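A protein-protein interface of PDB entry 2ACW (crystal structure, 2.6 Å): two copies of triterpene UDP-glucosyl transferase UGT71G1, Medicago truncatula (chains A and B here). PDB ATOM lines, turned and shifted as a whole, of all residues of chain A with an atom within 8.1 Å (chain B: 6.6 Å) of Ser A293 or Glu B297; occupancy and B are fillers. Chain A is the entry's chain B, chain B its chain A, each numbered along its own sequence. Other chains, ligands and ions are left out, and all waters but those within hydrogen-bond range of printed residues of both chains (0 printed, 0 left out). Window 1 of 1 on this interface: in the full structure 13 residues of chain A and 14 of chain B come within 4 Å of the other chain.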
ATOM      1  N   PHE A 290      26.475  -2.488   8.339  1.00  0.00           N
ATOM      2  CA  PHE A 290      25.991  -3.176   9.529  1.00  0.00           C
ATOM      3  C   PHE A 290      24.604  -2.618   9.777  1.00  0.00           C
ATOM      4  O   PHE A 290      24.298  -1.518   9.335  1.00  0.00           O
ATOM      5  CB  PHE A 290      26.846  -2.833  10.748  1.00  0.00           C
ATOM      6  CG  PHE A 290      28.196  -3.481  10.770  1.00  0.00           C
ATOM      7  CD1 PHE A 290      28.324  -4.851  10.942  1.00  0.00           C
ATOM      8  CD2 PHE A 290      29.346  -2.704  10.694  1.00  0.00           C
ATOM      9  CE1 PHE A 290      29.584  -5.443  11.048  1.00  0.00           C
ATOM     10  CE2 PHE A 290      30.613  -3.283  10.796  1.00  0.00           C
ATOM     11  CZ  PHE A 290      30.728  -4.662  10.975  1.00  0.00           C
ATOM     12  N   GLY A 291      23.772  -3.372  10.489  1.00  0.00           N
ATOM     13  CA  GLY A 291      22.436  -2.892  10.786  1.00  0.00           C
ATOM     14  C   GLY A 291      22.480  -1.717  11.749  1.00  0.00           C
ATOM     15  O   GLY A 291      23.534  -1.401  12.307  1.00  0.00           O
ATOM     16  N   PRO A 292      21.351  -1.038  11.958  1.00  0.00           N
ATOM     17  CA  PRO A 292      21.343   0.095  12.876  1.00  0.00           C
ATOM     18  C   PRO A 292      21.902  -0.236  14.259  1.00  0.00           C
ATOM     19  O   PRO A 292      22.776   0.478  14.764  1.00  0.00           O
ATOM     20  CB  PRO A 292      19.879   0.491  12.897  1.00  0.00           C
ATOM     21  CG  PRO A 292      19.485   0.252  11.453  1.00  0.00           C
ATOM     22  CD  PRO A 292      20.080  -1.122  11.217  1.00  0.00           C
ATOM     23  N   SER A 293      21.431  -1.318  14.868  1.00  0.00           N
ATOM     24  CA  SER A 293      21.926  -1.696  16.186  1.00  0.00           C
ATOM     25  C   SER A 293      23.436  -1.737  16.242  1.00  0.00           C
ATOM     26  O   SER A 293      24.049  -1.130  17.121  1.00  0.00           O
ATOM     27  CB  SER A 293      21.377  -3.048  16.611  1.00  0.00           C
ATOM     28  OG  SER A 293      20.033  -2.920  17.022  1.00  0.00           O
ATOM     29  N   GLN A 294      24.049  -2.449  15.308  1.00  0.00           N
ATOM     30  CA  GLN A 294      25.498  -2.543  15.301  1.00  0.00           C
ATOM     31  C   GLN A 294      26.131  -1.160  15.165  1.00  0.00           C
ATOM     32  O   GLN A 294      27.114  -0.856  15.839  1.00  0.00           O
ATOM     33  CB  GLN A 294      25.972  -3.463  14.178  1.00  0.00           C
ATOM     34  CG  GLN A 294      27.418  -3.851  14.357  1.00  0.00           C
ATOM     35  CD  GLN A 294      27.674  -4.520  15.697  1.00  0.00           C
ATOM     36  OE1 GLN A 294      27.654  -5.744  15.800  1.00  0.00           O
ATOM     37  NE2 GLN A 294      27.901  -3.714  16.733  1.00  0.00           N
ATOM     38  N   ILE A 295      25.567  -0.313  14.306  1.00  0.00           N
ATOM     39  CA  ILE A 295      26.107   1.042  14.146  1.00  0.00           C
ATOM     40  C   ILE A 295      26.055   1.831  15.471  1.00  0.00           C
ATOM     41  O   ILE A 295      27.043   2.421  15.888  1.00  0.00           O
ATOM     42  CB  ILE A 295      25.329   1.836  13.073  1.00  0.00           C
ATOM     43  CG1 ILE A 295      25.560   1.215  11.704  1.00  0.00           C
ATOM     44  CG2 ILE A 295      25.786   3.310  13.068  1.00  0.00           C
ATOM     45  CD1 ILE A 295      26.956   1.404  11.237  1.00  0.00           C
ATOM     46  N   ARG A 296      24.895   1.833  16.122  1.00  0.00           N
ATOM     47  CA  ARG A 296      24.746   2.550  17.379  1.00  0.00           C
ATOM     48  C   ARG A 296      25.722   2.047  18.424  1.00  0.00           C
ATOM     49  O   ARG A 296      26.265   2.831  19.208  1.00  0.00           O
ATOM     50  CB  ARG A 296      23.330   2.395  17.930  1.00  0.00           C
ATOM     51  CG  ARG A 296      22.274   3.189  17.222  1.00  0.00           C
ATOM     52  CD  ARG A 296      20.919   2.650  17.600  1.00  0.00           C
ATOM     53  NE  ARG A 296      20.008   2.802  16.486  1.00  0.00           N
ATOM     54  CZ  ARG A 296      19.145   1.880  16.100  1.00  0.00           C
ATOM     55  NH1 ARG A 296      19.063   0.728  16.740  1.00  0.00           N
ATOM     56  NH2 ARG A 296      18.374   2.105  15.056  1.00  0.00           N
ATOM     57  N   GLU A 297      25.918   0.733  18.453  1.00  0.00           N
ATOM     58  CA  GLU A 297      26.836   0.137  19.410  1.00  0.00           C
ATOM     59  C   GLU A 297      28.282   0.502  19.080  1.00  0.00           C
ATOM     60  O   GLU A 297      29.071   0.769  19.985  1.00  0.00           O
ATOM     61  CB  GLU A 297      26.655  -1.384  19.438  1.00  0.00           C
ATOM     62  CG  GLU A 297      25.339  -1.837  20.060  1.00  0.00           C
ATOM     63  CD  GLU A 297      25.238  -1.457  21.535  1.00  0.00           C
ATOM     64  OE1 GLU A 297      26.178  -1.795  22.288  1.00  0.00           O
ATOM     65  OE2 GLU A 297      24.232  -0.826  21.944  1.00  0.00           O
ATOM     66  N   ILE A 298      28.645   0.526  17.796  1.00  0.00           N
ATOM     67  CA  ILE A 298      30.011   0.894  17.439  1.00  0.00           C
ATOM     68  C   ILE A 298      30.208   2.362  17.794  1.00  0.00           C
ATOM     69  O   ILE A 298      31.275   2.752  18.254  1.00  0.00           O
ATOM     70  CB  ILE A 298      30.300   0.690  15.924  1.00  0.00           C
ATOM     71  CG1 ILE A 298      30.368  -0.803  15.592  1.00  0.00           C
ATOM     72  CG2 ILE A 298      31.605   1.405  15.521  1.00  0.00           C
ATOM     73  CD1 ILE A 298      30.581  -1.071  14.120  1.00  0.00           C
ATOM     74  N   ALA A 299      29.174   3.177  17.603  1.00  0.00           N
ATOM     75  CA  ALA A 299      29.272   4.601  17.921  1.00  0.00           C
ATOM     76  C   ALA A 299      29.492   4.829  19.411  1.00  0.00           C
ATOM     77  O   ALA A 299      30.413   5.528  19.790  1.00  0.00           O
ATOM     78  CB  ALA A 299      28.023   5.340  17.453  1.00  0.00           C
ATOM     79  N   LEU A 300      28.648   4.252  20.260  1.00  0.00           N
ATOM     80  CA  LEU A 300      28.807   4.411  21.704  1.00  0.00           C
ATOM     81  C   LEU A 300      30.179   3.915  22.104  1.00  0.00           C
ATOM     82  O   LEU A 300      30.891   4.580  22.861  1.00  0.00           O
ATOM     83  CB  LEU A 300      27.741   3.616  22.467  1.00  0.00           C
ATOM     84  CG  LEU A 300      27.683   3.775  23.994  1.00  0.00           C
ATOM     85  CD1 LEU A 300      27.749   5.264  24.372  1.00  0.00           C
ATOM     86  CD2 LEU A 300      26.413   3.151  24.529  1.00  0.00           C
ATOM     87  N   TRP A 311      35.794   7.278  10.988  1.00  0.00           N
ATOM     88  CA  TRP A 311      34.953   6.130  10.711  1.00  0.00           C
ATOM     89  C   TRP A 311      34.296   6.196   9.332  1.00  0.00           C
ATOM     90  O   TRP A 311      33.562   7.130   9.024  1.00  0.00           O
ATOM     91  CB  TRP A 311      33.910   6.034  11.840  1.00  0.00           C
ATOM     92  CG  TRP A 311      32.881   4.952  11.726  1.00  0.00           C
ATOM     93  CD1 TRP A 311      32.893   3.877  10.891  1.00  0.00           C
ATOM     94  CD2 TRP A 311      31.725   4.805  12.552  1.00  0.00           C
ATOM     95  NE1 TRP A 311      31.818   3.062  11.149  1.00  0.00           N
ATOM     96  CE2 TRP A 311      31.087   3.608  12.169  1.00  0.00           C
ATOM     97  CE3 TRP A 311      31.171   5.570  13.589  1.00  0.00           C
ATOM     98  CZ2 TRP A 311      29.919   3.150  12.790  1.00  0.00           C
ATOM     99  CZ3 TRP A 311      30.012   5.117  14.208  1.00  0.00           C
ATOM    100  CH2 TRP A 311      29.399   3.915  13.807  1.00  0.00           C
ATOM    101  N   VAL A 319      20.252   6.997  11.969  1.00  0.00           N
ATOM    102  CA  VAL A 319      20.550   5.750  12.640  1.00  0.00           C
ATOM    103  C   VAL A 319      21.371   5.929  13.914  1.00  0.00           C
ATOM    104  O   VAL A 319      21.149   5.229  14.895  1.00  0.00           O
ATOM    105  CB  VAL A 319      21.294   4.795  11.658  1.00  0.00           C
ATOM    106  CG1 VAL A 319      22.138   3.773  12.421  1.00  0.00           C
ATOM    107  CG2 VAL A 319      20.281   4.099  10.772  1.00  0.00           C
ATOM    108  N   PRO A 321      23.080   7.159  17.515  1.00  0.00           N
ATOM    109  CA  PRO A 321      22.519   7.469  18.828  1.00  0.00           C
ATOM    110  C   PRO A 321      22.334   8.967  18.898  1.00  0.00           C
ATOM    111  O   PRO A 321      23.090   9.707  18.276  1.00  0.00           O
ATOM    112  CB  PRO A 321      23.606   6.998  19.790  1.00  0.00           C
ATOM    113  CG  PRO A 321      24.325   5.969  19.028  1.00  0.00           C
ATOM    114  CD  PRO A 321      24.418   6.571  17.665  1.00  0.00           C
ATOM    115  N   VAL A 409      24.931  -8.923  17.574  1.00  0.00           N
ATOM    116  CA  VAL A 409      25.624  -7.641  17.563  1.00  0.00           C
ATOM    117  C   VAL A 409      26.733  -7.589  18.609  1.00  0.00           C
ATOM    118  O   VAL A 409      26.609  -8.158  19.696  1.00  0.00           O
ATOM    119  CB  VAL A 409      24.655  -6.433  17.800  1.00  0.00           C
ATOM    120  CG1 VAL A 409      23.257  -6.743  17.249  1.00  0.00           C
ATOM    121  CG2 VAL A 409      24.601  -6.066  19.255  1.00  0.00           C
ATOM    122  N   VAL A 410      27.825  -6.919  18.258  1.00  0.00           N
ATOM    123  CA  VAL A 410      28.952  -6.755  19.158  1.00  0.00           C
ATOM    124  C   VAL A 410      28.673  -5.520  20.030  1.00  0.00           C
ATOM    125  O   VAL A 410      28.528  -4.407  19.529  1.00  0.00           O
ATOM    126  CB  VAL A 410      30.251  -6.560  18.370  1.00  0.00           C
ATOM    127  CG1 VAL A 410      31.401  -6.315  19.324  1.00  0.00           C
ATOM    128  CG2 VAL A 410      30.526  -7.784  17.522  1.00  0.00           C
ATOM    129  N   ALA A 411      28.603  -5.729  21.337  1.00  0.00           N
ATOM    130  CA  ALA A 411      28.291  -4.666  22.281  1.00  0.00           C
ATOM    131  C   ALA A 411      29.349  -3.591  22.431  1.00  0.00           C
ATOM    132  O   ALA A 411      30.542  -3.873  22.401  1.00  0.00           O
ATOM    133  CB  ALA A 411      27.985  -5.276  23.639  1.00  0.00           C
ATOM    134  N   ALA A 412      28.896  -2.352  22.603  1.00  0.00           N
ATOM    135  CA  ALA A 412      29.795  -1.218  22.785  1.00  0.00           C
ATOM    136  C   ALA A 412      30.891  -1.510  23.820  1.00  0.00           C
ATOM    137  O   ALA A 412      32.030  -1.064  23.665  1.00  0.00           O
ATOM    138  CB  ALA A 412      29.002  -0.004  23.200  1.00  0.00           C
ATOM    139  N   ILE A 415      33.651  -3.502  22.106  1.00  0.00           N
ATOM    140  CA  ILE A 415      34.327  -2.591  21.178  1.00  0.00           C
ATOM    141  C   ILE A 415      35.257  -1.641  21.921  1.00  0.00           C
ATOM    142  O   ILE A 415      36.434  -1.534  21.603  1.00  0.00           O
ATOM    143  CB  ILE A 415      33.307  -1.769  20.351  1.00  0.00           C
ATOM    144  CG1 ILE A 415      32.484  -2.710  19.466  1.00  0.00           C
ATOM    145  CG2 ILE A 415      34.025  -0.734  19.509  1.00  0.00           C
ATOM    146  CD1 ILE A 415      31.286  -2.068  18.869  1.00  0.00           C
ATOM    147  N   PRO B 292      23.116  -5.133  28.057  1.00  0.00           N
ATOM    148  CA  PRO B 292      23.267  -3.694  27.818  1.00  0.00           C
ATOM    149  C   PRO B 292      22.793  -3.214  26.457  1.00  0.00           C
ATOM    150  O   PRO B 292      21.977  -2.285  26.376  1.00  0.00           O
ATOM    151  CB  PRO B 292      24.758  -3.460  28.034  1.00  0.00           C
ATOM    152  CG  PRO B 292      25.102  -4.491  29.055  1.00  0.00           C
ATOM    153  CD  PRO B 292      24.394  -5.711  28.494  1.00  0.00           C
ATOM    154  N   SER B 293      23.300  -3.843  25.397  1.00  0.00           N
ATOM    155  CA  SER B 293      22.924  -3.489  24.030  1.00  0.00           C
ATOM    156  C   SER B 293      21.415  -3.593  23.828  1.00  0.00           C
ATOM    157  O   SER B 293      20.794  -2.693  23.248  1.00  0.00           O
ATOM    158  CB  SER B 293      23.640  -4.402  23.041  1.00  0.00           C
ATOM    159  OG  SER B 293      23.390  -5.753  23.372  1.00  0.00           O
ATOM    160  N   GLN B 294      20.816  -4.684  24.299  1.00  0.00           N
ATOM    161  CA  GLN B 294      19.376  -4.839  24.161  1.00  0.00           C
ATOM    162  C   GLN B 294      18.624  -3.764  24.948  1.00  0.00           C
ATOM    163  O   GLN B 294      17.597  -3.259  24.496  1.00  0.00           O
ATOM    164  CB  GLN B 294      18.914  -6.206  24.652  1.00  0.00           C
ATOM    165  CG  GLN B 294      17.411  -6.385  24.485  1.00  0.00           C
ATOM    166  CD  GLN B 294      17.024  -6.506  23.040  1.00  0.00           C
ATOM    167  OE1 GLN B 294      17.234  -7.553  22.423  1.00  0.00           O
ATOM    168  NE2 GLN B 294      16.478  -5.436  22.479  1.00  0.00           N
ATOM    169  N   ILE B 295      19.124  -3.436  26.136  1.00  0.00           N
ATOM    170  CA  ILE B 295      18.490  -2.414  26.955  1.00  0.00           C
ATOM    171  C   ILE B 295      18.440  -1.097  26.186  1.00  0.00           C
ATOM    172  O   ILE B 295      17.376  -0.484  26.056  1.00  0.00           O
ATOM    173  CB  ILE B 295      19.262  -2.164  28.286  1.00  0.00           C
ATOM    174  CG1 ILE B 295      19.111  -3.365  29.221  1.00  0.00           C
ATOM    175  CG2 ILE B 295      18.715  -0.896  28.981  1.00  0.00           C
ATOM    176  CD1 ILE B 295      17.743  -3.461  29.864  1.00  0.00           C
ATOM    177  N   ARG B 296      19.602  -0.677  25.686  1.00  0.00           N
ATOM    178  CA  ARG B 296      19.712   0.573  24.945  1.00  0.00           C
ATOM    179  C   ARG B 296      18.754   0.590  23.762  1.00  0.00           C
ATOM    180  O   ARG B 296      18.127   1.613  23.472  1.00  0.00           O
ATOM    181  CB  ARG B 296      21.137   0.783  24.447  1.00  0.00           C
ATOM    182  CG  ARG B 296      22.200   0.704  25.511  1.00  0.00           C
ATOM    183  CD  ARG B 296      23.567   1.024  24.924  1.00  0.00           C
ATOM    184  NE  ARG B 296      24.636   0.561  25.800  1.00  0.00           N
ATOM    185  CZ  ARG B 296      25.317  -0.567  25.627  1.00  0.00           C
ATOM    186  NH1 ARG B 296      25.061  -1.363  24.602  1.00  0.00           N
ATOM    187  NH2 ARG B 296      26.253  -0.906  26.499  1.00  0.00           N
ATOM    188  N   GLU B 297      18.636  -0.542  23.083  1.00  0.00           N
ATOM    189  CA  GLU B 297      17.732  -0.630  21.945  1.00  0.00           C
ATOM    190  C   GLU B 297      16.285  -0.425  22.370  1.00  0.00           C
ATOM    191  O   GLU B 297      15.507   0.226  21.666  1.00  0.00           O
ATOM    192  CB  GLU B 297      17.893  -1.985  21.246  1.00  0.00           C
ATOM    193  CG  GLU B 297      19.211  -2.116  20.516  1.00  0.00           C
ATOM    194  CD  GLU B 297      19.266  -1.205  19.316  1.00  0.00           C
ATOM    195  OE1 GLU B 297      18.320  -1.276  18.503  1.00  0.00           O
ATOM    196  OE2 GLU B 297      20.235  -0.428  19.186  1.00  0.00           O
ATOM    197  N   ILE B 298      15.907  -0.996  23.509  1.00  0.00           N
ATOM    198  CA  ILE B 298      14.550  -0.808  23.992  1.00  0.00           C
ATOM    199  C   ILE B 298      14.376   0.681  24.343  1.00  0.00           C
ATOM    200  O   ILE B 298      13.383   1.295  23.975  1.00  0.00           O
ATOM    201  CB  ILE B 298      14.263  -1.705  25.237  1.00  0.00           C
ATOM    202  CG1 ILE B 298      14.255  -3.177  24.816  1.00  0.00           C
ATOM    203  CG2 ILE B 298      12.931  -1.316  25.882  1.00  0.00           C
ATOM    204  CD1 ILE B 298      14.122  -4.157  25.961  1.00  0.00           C
ATOM    205  N   ALA B 299      15.352   1.261  25.035  1.00  0.00           N
ATOM    206  CA  ALA B 299      15.289   2.670  25.422  1.00  0.00           C
ATOM    207  C   ALA B 299      15.115   3.612  24.229  1.00  0.00           C
ATOM    208  O   ALA B 299      14.358   4.582  24.298  1.00  0.00           O
ATOM    209  CB  ALA B 299      16.534   3.053  26.202  1.00  0.00           C
ATOM    210  N   LEU B 300      15.823   3.335  23.140  1.00  0.00           N
ATOM    211  CA  LEU B 300      15.724   4.164  21.943  1.00  0.00           C
ATOM    212  C   LEU B 300      14.398   3.908  21.257  1.00  0.00           C
ATOM    213  O   LEU B 300      13.764   4.826  20.754  1.00  0.00           O
ATOM    214  CB  LEU B 300      16.844   3.838  20.970  1.00  0.00           C
ATOM    215  CG  LEU B 300      16.854   4.727  19.719  1.00  0.00           C
ATOM    216  CD1 LEU B 300      17.550   6.042  20.053  1.00  0.00           C
ATOM    217  CD2 LEU B 300      17.570   4.016  18.575  1.00  0.00           C
ATOM    218  N   GLY B 301      13.993   2.643  21.229  1.00  0.00           N
ATOM    219  CA  GLY B 301      12.733   2.275  20.612  1.00  0.00           C
ATOM    220  C   GLY B 301      11.559   2.951  21.291  1.00  0.00           C
ATOM    221  O   GLY B 301      10.636   3.410  20.624  1.00  0.00           O
ATOM    222  N   LEU B 302      11.588   3.017  22.620  1.00  0.00           N
ATOM    223  CA  LEU B 302      10.506   3.649  23.359  1.00  0.00           C
ATOM    224  C   LEU B 302      10.426   5.138  23.047  1.00  0.00           C
ATOM    225  O   LEU B 302       9.336   5.673  22.848  1.00  0.00           O
ATOM    226  CB  LEU B 302      10.688   3.443  24.869  1.00  0.00           C
ATOM    227  CG  LEU B 302      10.361   2.048  25.441  1.00  0.00           C
ATOM    228  CD1 LEU B 302      11.020   1.872  26.798  1.00  0.00           C
ATOM    229  CD2 LEU B 302       8.861   1.857  25.527  1.00  0.00           C
ATOM    230  N   TRP B 311       8.572   1.375  32.431  1.00  0.00           N
ATOM    231  CA  TRP B 311       9.496   0.293  32.193  1.00  0.00           C
ATOM    232  C   TRP B 311      10.058  -0.302  33.483  1.00  0.00           C
ATOM    233  O   TRP B 311      10.794   0.356  34.236  1.00  0.00           O
ATOM    234  CB  TRP B 311      10.632   0.830  31.338  1.00  0.00           C
ATOM    235  CG  TRP B 311      11.599  -0.193  30.800  1.00  0.00           C
ATOM    236  CD1 TRP B 311      11.624  -1.532  31.060  1.00  0.00           C
ATOM    237  CD2 TRP B 311      12.705   0.069  29.931  1.00  0.00           C
ATOM    238  NE1 TRP B 311      12.680  -2.115  30.412  1.00  0.00           N
ATOM    239  CE2 TRP B 311      13.362  -1.156  29.711  1.00  0.00           C
ATOM    240  CE3 TRP B 311      13.205   1.227  29.321  1.00  0.00           C
ATOM    241  CZ2 TRP B 311      14.499  -1.264  28.906  1.00  0.00           C
ATOM    242  CZ3 TRP B 311      14.342   1.120  28.518  1.00  0.00           C
ATOM    243  CH2 TRP B 311      14.973  -0.119  28.319  1.00  0.00           C
ATOM    244  N   PRO B 321      21.252   4.745  26.872  1.00  0.00           N
ATOM    245  CA  PRO B 321      21.766   5.695  25.875  1.00  0.00           C
ATOM    246  C   PRO B 321      22.070   7.016  26.572  1.00  0.00           C
ATOM    247  O   PRO B 321      21.290   7.458  27.412  1.00  0.00           O
ATOM    248  CB  PRO B 321      20.600   5.834  24.894  1.00  0.00           C
ATOM    249  CG  PRO B 321      19.920   4.507  24.971  1.00  0.00           C
ATOM    250  CD  PRO B 321      19.944   4.198  26.462  1.00  0.00           C
ATOM    251  N   VAL B 409      19.731  -9.327  19.263  1.00  0.00           N
ATOM    252  CA  VAL B 409      19.088  -8.228  19.946  1.00  0.00           C
ATOM    253  C   VAL B 409      17.967  -7.724  19.033  1.00  0.00           C
ATOM    254  O   VAL B 409      18.140  -7.652  17.819  1.00  0.00           O
ATOM    255  CB  VAL B 409      20.062  -7.063  20.218  1.00  0.00           C
ATOM    256  CG1 VAL B 409      21.440  -7.610  20.569  1.00  0.00           C
ATOM    257  CG2 VAL B 409      20.117  -6.131  19.037  1.00  0.00           C
ATOM    258  N   VAL B 410      16.813  -7.417  19.624  1.00  0.00           N
ATOM    259  CA  VAL B 410      15.677  -6.894  18.890  1.00  0.00           C
ATOM    260  C   VAL B 410      15.927  -5.399  18.821  1.00  0.00           C
ATOM    261  O   VAL B 410      16.023  -4.731  19.852  1.00  0.00           O
ATOM    262  CB  VAL B 410      14.381  -7.150  19.634  1.00  0.00           C
ATOM    263  CG1 VAL B 410      13.206  -6.504  18.882  1.00  0.00           C
ATOM    264  CG2 VAL B 410      14.186  -8.621  19.790  1.00  0.00           C
ATOM    265  N   ALA B 411      16.024  -4.890  17.599  1.00  0.00           N
ATOM    266  CA  ALA B 411      16.326  -3.491  17.330  1.00  0.00           C
ATOM    267  C   ALA B 411      15.201  -2.500  17.529  1.00  0.00           C
ATOM    268  O   ALA B 411      14.033  -2.819  17.344  1.00  0.00           O
ATOM    269  CB  ALA B 411      16.865  -3.365  15.923  1.00  0.00           C
ATOM    270  N   ALA B 412      15.586  -1.279  17.889  1.00  0.00           N
ATOM    271  CA  ALA B 412      14.655  -0.182  18.121  1.00  0.00           C
ATOM    272  C   ALA B 412      13.643  -0.002  16.995  1.00  0.00           C
ATOM    273  O   ALA B 412      12.472   0.243  17.258  1.00  0.00           O
ATOM    274  CB  ALA B 412      15.429   1.106  18.327  1.00  0.00           C
ATOM    275  N   GLU B 413      14.080  -0.106  15.743  1.00  0.00           N
ATOM    276  CA  GLU B 413      13.145   0.051  14.629  1.00  0.00           C
ATOM    277  C   GLU B 413      12.009  -0.968  14.708  1.00  0.00           C
ATOM    278  O   GLU B 413      10.859  -0.660  14.404  1.00  0.00           O
ATOM    279  CB  GLU B 413      13.843  -0.133  13.278  1.00  0.00           C
ATOM    280  CG  GLU B 413      14.745   0.993  12.829  1.00  0.00           C
ATOM    281  CD  GLU B 413      15.962   1.157  13.697  1.00  0.00           C
ATOM    282  OE1 GLU B 413      16.552   0.133  14.128  1.00  0.00           O
ATOM    283  OE2 GLU B 413      16.339   2.322  13.926  1.00  0.00           O
ATOM    284  N   ILE B 415      11.064  -2.604  17.513  1.00  0.00           N
ATOM    285  CA  ILE B 415      10.332  -2.309  18.745  1.00  0.00           C
ATOM    286  C   ILE B 415       9.357  -1.143  18.539  1.00  0.00           C
ATOM    287  O   ILE B 415       8.198  -1.208  18.938  1.00  0.00           O
ATOM    288  CB  ILE B 415      11.319  -1.943  19.878  1.00  0.00           C
ATOM    289  CG1 ILE B 415      12.114  -3.185  20.285  1.00  0.00           C
ATOM    290  CG2 ILE B 415      10.581  -1.338  21.037  1.00  0.00           C
ATOM    291  CD1 ILE B 415      13.351  -2.889  21.101  1.00  0.00           C
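Ser A293 touches Val B409, but with the chains exchanged Val A409 does not touch Ser B293 (4.2 Å).
Arg A296 touches Glu B297, and with the chains exchanged Glu A297 touches Arg B296.
Arg A296 touches Leu B300, and with the chains exchanged Leu A300 touches Arg B296.
Arg A296 touches Ala B412, but with the chains exchanged Ala A412 does not touch Arg B296 (4.4 Å).
Positions printed for both chains: 292, 293, 294, 295, 296, 297, 298, 299, 300, 311, 321, 409, 410, 411, 412 and 415.
Of the 12 pairs that touch across the chains among the printed residues, 7 have their exchanged pair printed and touching as well.
Hydrophobic or aromatic side chains of chain A that line the printed part of chain B: Pro A292, Leu A300 and Val A409.
Along chain A the printed residues that touch a printed residue of chain B span positions 292 to 409.
Of the 19 printed residues of chain B, 8 touch a printed residue of chain A.
Printed residues of chain B that touch a printed residue of chain A: Ser B293, Arg B296, Glu B297, Leu B300, Val B409, Ala B411, Ala B412 and Glu B413.
Among the printed residues, Asp or Glu carboxylates within 4 Å of a Lys or Arg side-chain nitrogen of the other chain: Arg A296 with Glu B297 (2.8 Å), Arg A296 with Glu B413 (2.3 Å) and Glu A297 with Arg B296 (2.6 Å).
N of Ala B412 is in hydrogen-bond range of OE1 of Glu B297 (2.8 Å).
The backbone carbonyl oxygen of Val A319 is in hydrogen-bond range of the guanidinium group of Arg A296.
N of Ala A412 sits at hydrogen-bond distance from OE1 of Glu A297 (2.8 Å).
Ser A293 touches just these residues of chain B: Glu B297 (2.8 Å), Val B409 (3.8 Å) and Ala B411 (3.4 Å).
Glu B297 touches just these residues of chain A: Ser A293 (2.8 Å) and Arg A296 (2.8 Å).
Printed residues of chain A within 4 Å of Val B409: Ser A293 and Val A409.
Printed residues of chain B within 4 Å of Pro A292: Glu B413 (3.6 Å).
The nearest residue of chain B that does not touch Ser A293 is Ala B412 (4.8 Å).
The nearest printed residue of chain B that does not touch Glu A297 is Glu B297 (4.9 Å).
NH1 of Arg B296 lies within salt-bridge range of OE1 of Glu A297 (2.6 Å).
The side-chain hydroxyl of Ser A293 is in hydrogen-bond range of the side-chain carboxylate of Glu B297.
The side-chain carboxylate (OE1) of Glu B297 lies within salt-bridge range of the guanidinium group (NH1) of Arg A296 (2.8 Å).
The side-chain carboxylate of Glu B413 lies within salt-bridge range of the guanidinium group of Arg A296.
Among the printed residues, merely in contact across the chains: Pro A292 with Glu B413, Ser A293 with Val B409, Ser A293 with Ala B411, Arg A296 with Leu B300, Arg A296 with Ala B412, Glu A297 with Ser B293, Leu A300 with Arg B296 and Val A409 with Val B409.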
